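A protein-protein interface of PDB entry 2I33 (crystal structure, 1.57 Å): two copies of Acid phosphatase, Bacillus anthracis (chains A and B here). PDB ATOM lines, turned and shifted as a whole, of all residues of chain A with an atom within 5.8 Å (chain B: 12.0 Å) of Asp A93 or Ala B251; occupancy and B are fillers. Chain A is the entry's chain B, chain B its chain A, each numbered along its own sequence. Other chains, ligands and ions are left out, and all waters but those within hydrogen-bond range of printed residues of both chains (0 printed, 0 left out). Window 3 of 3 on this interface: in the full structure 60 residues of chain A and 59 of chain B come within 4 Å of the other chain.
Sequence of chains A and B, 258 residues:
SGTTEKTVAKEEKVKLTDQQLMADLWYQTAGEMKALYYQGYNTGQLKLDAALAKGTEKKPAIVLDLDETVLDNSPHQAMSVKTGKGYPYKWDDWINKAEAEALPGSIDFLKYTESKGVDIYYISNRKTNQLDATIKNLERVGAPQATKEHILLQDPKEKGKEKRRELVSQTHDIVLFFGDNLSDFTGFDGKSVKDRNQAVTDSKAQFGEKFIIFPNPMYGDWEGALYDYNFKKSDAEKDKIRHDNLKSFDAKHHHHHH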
ATOM      1  N   MET A  79       2.269   0.838  -6.258  1.00  0.00           N
ATOM      2  CA  MET A  79       3.458   0.011  -6.468  1.00  0.00           C
ATOM      3  C   MET A  79       4.697   0.898  -6.609  1.00  0.00           C
ATOM      4  O   MET A  79       5.719   0.643  -5.979  1.00  0.00           O
ATOM      5  CB  MET A  79       3.234  -0.870  -7.701  1.00  0.00           C
ATOM      6  CG  MET A  79       4.379  -1.771  -8.078  1.00  0.00           C
ATOM      7  SD  MET A  79       5.692  -0.878  -8.928  1.00  0.00           S
ATOM      8  CE  MET A  79       4.874  -0.323 -10.419  1.00  0.00           C
ATOM      9  N   LYS A  90       7.118  -0.787 -14.801  1.00  0.00           N
ATOM     10  CA  LYS A  90       5.977  -1.713 -14.790  1.00  0.00           C
ATOM     11  C   LYS A  90       4.634  -1.132 -15.250  1.00  0.00           C
ATOM     12  O   LYS A  90       3.579  -1.750 -15.065  1.00  0.00           O
ATOM     13  CB  LYS A  90       5.840  -2.395 -13.415  1.00  0.00           C
ATOM     14  CG  LYS A  90       6.893  -3.470 -13.113  1.00  0.00           C
ATOM     15  CD  LYS A  90       7.099  -4.445 -14.274  1.00  0.00           C
ATOM     16  CE  LYS A  90       8.025  -5.604 -13.935  1.00  0.00           C
ATOM     17  NZ  LYS A  90       7.920  -6.635 -14.996  1.00  0.00           N
ATOM     18  N   TRP A  91       4.649   0.045 -15.880  1.00  0.00           N
ATOM     19  CA  TRP A  91       3.408   0.590 -16.433  1.00  0.00           C
ATOM     20  C   TRP A  91       2.847  -0.307 -17.532  1.00  0.00           C
ATOM     21  O   TRP A  91       1.676  -0.659 -17.508  1.00  0.00           O
ATOM     22  CB  TRP A  91       3.603   2.021 -16.961  1.00  0.00           C
ATOM     23  CG  TRP A  91       2.359   2.572 -17.532  1.00  0.00           C
ATOM     24  CD1 TRP A  91       2.062   2.736 -18.851  1.00  0.00           C
ATOM     25  CD2 TRP A  91       1.195   2.951 -16.803  1.00  0.00           C
ATOM     26  NE1 TRP A  91       0.795   3.250 -18.983  1.00  0.00           N
ATOM     27  CE2 TRP A  91       0.238   3.394 -17.740  1.00  0.00           C
ATOM     28  CE3 TRP A  91       0.883   3.026 -15.440  1.00  0.00           C
ATOM     29  CZ2 TRP A  91      -1.027   3.855 -17.361  1.00  0.00           C
ATOM     30  CZ3 TRP A  91      -0.360   3.483 -15.063  1.00  0.00           C
ATOM     31  CH2 TRP A  91      -1.310   3.906 -16.021  1.00  0.00           C
ATOM     32  N   ASP A  92       3.663  -0.669 -18.507  1.00  0.00           N
ATOM     33  CA  ASP A  92       3.147  -1.487 -19.600  1.00  0.00           C
ATOM     34  C   ASP A  92       2.687  -2.865 -19.113  1.00  0.00           C
ATOM     35  O   ASP A  92       1.681  -3.385 -19.596  1.00  0.00           O
ATOM     36  CB  ASP A  92       4.167  -1.589 -20.720  1.00  0.00           C
ATOM     37  CG  ASP A  92       4.460  -0.240 -21.382  1.00  0.00           C
ATOM     38  OD1 ASP A  92       3.656   0.708 -21.240  1.00  0.00           O
ATOM     39  OD2 ASP A  92       5.496  -0.169 -22.086  1.00  0.00           O
ATOM     40  N   ASP A  93       3.409  -3.424 -18.144  1.00  0.00           N
ATOM     41  CA  ASP A  93       3.046  -4.681 -17.481  1.00  0.00           C
ATOM     42  C   ASP A  93       1.630  -4.534 -16.909  1.00  0.00           C
ATOM     43  O   ASP A  93       0.757  -5.372 -17.102  1.00  0.00           O
ATOM     44  CB  ASP A  93       4.070  -4.942 -16.360  1.00  0.00           C
ATOM     45  CG  ASP A  93       3.918  -6.300 -15.682  1.00  0.00           C
ATOM     46  OD1 ASP A  93       2.797  -6.822 -15.573  1.00  0.00           O
ATOM     47  OD2 ASP A  93       4.949  -6.843 -15.222  1.00  0.00           O
ATOM     48  N   TRP A  94       1.439  -3.457 -16.169  1.00  0.00           N
ATOM     49  CA  TRP A  94       0.166  -3.192 -15.550  1.00  0.00           C
ATOM     50  C   TRP A  94      -0.925  -3.105 -16.608  1.00  0.00           C
ATOM     51  O   TRP A  94      -1.982  -3.746 -16.471  1.00  0.00           O
ATOM     52  CB  TRP A  94       0.257  -1.886 -14.741  1.00  0.00           C
ATOM     53  CG  TRP A  94      -1.052  -1.321 -14.369  1.00  0.00           C
ATOM     54  CD1 TRP A  94      -1.675  -0.231 -14.906  1.00  0.00           C
ATOM     55  CD2 TRP A  94      -1.938  -1.852 -13.398  1.00  0.00           C
ATOM     56  NE1 TRP A  94      -2.911  -0.054 -14.321  1.00  0.00           N
ATOM     57  CE2 TRP A  94      -3.092  -1.037 -13.383  1.00  0.00           C
ATOM     58  CE3 TRP A  94      -1.873  -2.946 -12.529  1.00  0.00           C
ATOM     59  CZ2 TRP A  94      -4.167  -1.285 -12.532  1.00  0.00           C
ATOM     60  CZ3 TRP A  94      -2.953  -3.193 -11.690  1.00  0.00           C
ATOM     61  CH2 TRP A  94      -4.074  -2.371 -11.699  1.00  0.00           C
ATOM     62  N   ILE A  95      -0.682  -2.320 -17.655  1.00  0.00           N
ATOM     63  CA  ILE A  95      -1.694  -2.165 -18.719  1.00  0.00           C
ATOM     64  C   ILE A  95      -2.034  -3.546 -19.300  1.00  0.00           C
ATOM     65  O   ILE A  95      -3.191  -3.905 -19.476  1.00  0.00           O
ATOM     66  CB  ILE A  95      -1.207  -1.226 -19.859  1.00  0.00           C
ATOM     67  CG1 ILE A  95      -1.125   0.235 -19.381  1.00  0.00           C
ATOM     68  CG2 ILE A  95      -2.116  -1.340 -21.101  1.00  0.00           C
ATOM     69  CD1 ILE A  95      -2.390   0.850 -18.846  1.00  0.00           C
ATOM     70  N   ASN A  96      -1.014  -4.328 -19.594  1.00  0.00           N
ATOM     71  CA  ASN A  96      -1.201  -5.642 -20.187  1.00  0.00           C
ATOM     72  C   ASN A  96      -2.002  -6.613 -19.307  1.00  0.00           C
ATOM     73  O   ASN A  96      -2.716  -7.494 -19.806  1.00  0.00           O
ATOM     74  CB  ASN A  96       0.171  -6.232 -20.484  1.00  0.00           C
ATOM     75  CG  ASN A  96       0.096  -7.426 -21.377  1.00  0.00           C
ATOM     76  OD1 ASN A  96      -0.336  -7.324 -22.524  1.00  0.00           O
ATOM     77  ND2 ASN A  96       0.486  -8.573 -20.856  1.00  0.00           N
ATOM     78  N   LYS A  97      -1.865  -6.465 -17.993  1.00  0.00           N
ATOM     79  CA  LYS A  97      -2.579  -7.337 -17.056  1.00  0.00           C
ATOM     80  C   LYS A  97      -4.085  -7.088 -17.174  1.00  0.00           C
ATOM     81  O   LYS A  97      -4.887  -7.963 -16.826  1.00  0.00           O
ATOM     82  CB  LYS A  97      -2.101  -7.109 -15.615  1.00  0.00           C
ATOM     83  N   ALA A  98      -4.455  -5.899 -17.662  1.00  0.00           N
ATOM     84  CA  ALA A  98      -5.849  -5.575 -17.954  1.00  0.00           C
ATOM     85  C   ALA A  98      -6.734  -5.882 -16.763  1.00  0.00           C
ATOM     86  O   ALA A  98      -7.818  -6.445 -16.918  1.00  0.00           O
ATOM     87  CB  ALA A  98      -6.325  -6.336 -19.182  1.00  0.00           C
ATOM     88  N   LYS B 247      -2.768  -0.053  -1.899  1.00  0.00           N
ATOM     89  CA  LYS B 247      -3.151  -1.306  -2.548  1.00  0.00           C
ATOM     90  C   LYS B 247      -2.285  -1.357  -3.787  1.00  0.00           C
ATOM     91  O   LYS B 247      -2.583  -0.716  -4.788  1.00  0.00           O
ATOM     92  CB  LYS B 247      -4.633  -1.306  -2.941  1.00  0.00           C
ATOM     93  CG  LYS B 247      -5.596  -0.836  -1.850  1.00  0.00           C
ATOM     94  N   SER B 248      -1.198  -2.109  -3.703  1.00  0.00           N
ATOM     95  CA  SER B 248      -0.188  -2.088  -4.746  1.00  0.00           C
ATOM     96  C   SER B 248      -0.331  -3.232  -5.745  1.00  0.00           C
ATOM     97  O   SER B 248      -0.734  -4.347  -5.405  1.00  0.00           O
ATOM     98  CB  SER B 248       1.209  -2.126  -4.123  1.00  0.00           C
ATOM     99  OG  SER B 248       1.321  -3.203  -3.217  1.00  0.00           O
ATOM    100  N   PHE B 249       0.033  -2.926  -6.978  1.00  0.00           N
ATOM    101  CA  PHE B 249       0.188  -3.879  -8.049  1.00  0.00           C
ATOM    102  C   PHE B 249       1.427  -4.720  -7.742  1.00  0.00           C
ATOM    103  O   PHE B 249       2.516  -4.172  -7.572  1.00  0.00           O
ATOM    104  CB  PHE B 249       0.369  -3.073  -9.341  1.00  0.00           C
ATOM    105  CG  PHE B 249       0.819  -3.860 -10.515  1.00  0.00           C
ATOM    106  CD1 PHE B 249       0.259  -5.096 -10.811  1.00  0.00           C
ATOM    107  CD2 PHE B 249       1.786  -3.340 -11.366  1.00  0.00           C
ATOM    108  CE1 PHE B 249       0.660  -5.803 -11.925  1.00  0.00           C
ATOM    109  CE2 PHE B 249       2.187  -4.043 -12.469  1.00  0.00           C
ATOM    110  CZ  PHE B 249       1.631  -5.280 -12.752  1.00  0.00           C
ATOM    111  N   ASP B 250       1.243  -6.030  -7.618  1.00  0.00           N
ATOM    112  CA  ASP B 250       2.369  -6.954  -7.483  1.00  0.00           C
ATOM    113  C   ASP B 250       2.655  -7.539  -8.866  1.00  0.00           C
ATOM    114  O   ASP B 250       1.950  -8.445  -9.327  1.00  0.00           O
ATOM    115  CB  ASP B 250       2.062  -8.061  -6.470  1.00  0.00           C
ATOM    116  CG  ASP B 250       3.210  -9.051  -6.316  1.00  0.00           C
ATOM    117  OD1 ASP B 250       4.376  -8.684  -6.578  1.00  0.00           O
ATOM    118  OD2 ASP B 250       2.946 -10.210  -5.929  1.00  0.00           O
ATOM    119  N   ALA B 251       3.684  -7.001  -9.522  1.00  0.00           N
ATOM    120  CA  ALA B 251       4.009  -7.370 -10.904  1.00  0.00           C
ATOM    121  C   ALA B 251       4.543  -8.790 -10.987  1.00  0.00           C
ATOM    122  O   ALA B 251       5.203  -9.264 -10.063  1.00  0.00           O
ATOM    123  CB  ALA B 251       5.020  -6.391 -11.482  1.00  0.00           C
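OD2 of Asp A93 lies within salt-bridge range of NZ of Lys A90 (3.0 Å).
Among the printed residues, pairs that only touch across the chains: Met A79 with Phe B249 (3.1 Å), Asp A93 with Phe B249 (3.4 Å), Trp A94 with Phe B249 (3.5 Å), Lys A90 with Phe B249 (3.7 Å), Asp A93 with Ala B251 (3.8 Å), Met A79 with Ser B248 (3.8 Å) and Lys A90 with Ala B251 (3.8 Å).
Printed residues of chain B within 4 Å of Asp A93: Phe B249 and Ala B251.
Printed residues of chain A within 4 Å of Ala B251: Lys A90 (3.8 Å) and Asp A93 (3.8 Å).
Asp A92 touches none of the printed residues of chain B.
Of the printed residues of chain B, Trp A94 touches Phe B249 (3.5 Å).
No residue of chain B comes within 4 Å of Ile A95.
Printed residues of chain B within 4 Å of Lys A90: Phe B249 and Ala B251.
Of the printed residues of chain B, Met A79 touches Ser B248 (3.8 Å) and Phe B249 (3.1 Å).
Lys B247 touches none of the printed residues of chain A.
The nearest printed residue of chain B that does not touch Asp A93 is Asp B250 (6.5 Å).
The nearest printed residue of chain A that does not touch Ala B251 is Met A79 (5.5 Å).
The nearest printed residue of chain A that does not touch Ser B248 is Trp A94 (6.5 Å).
Printed residues of chain A that touch a printed residue of chain B: Met A79, Lys A90, Asp A93 and Trp A94.
Hydrophobic or aromatic side chains of chain A within 4 Å of the printed part of chain B: Met A79 and Trp A94.
Hydrophobic or aromatic side chains of chain B that line the printed part of chain A: Phe B249 and Ala B251.
Along chain B the printed residues that touch a printed residue of chain A span positions 248 to 251.
Among the printed residues, 7 pairs touch across the chains.
No position is printed for both chains.
Of the 7 pairs that touch across the chains among the printed residues, none has its exchanged pair printed and touching as well.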
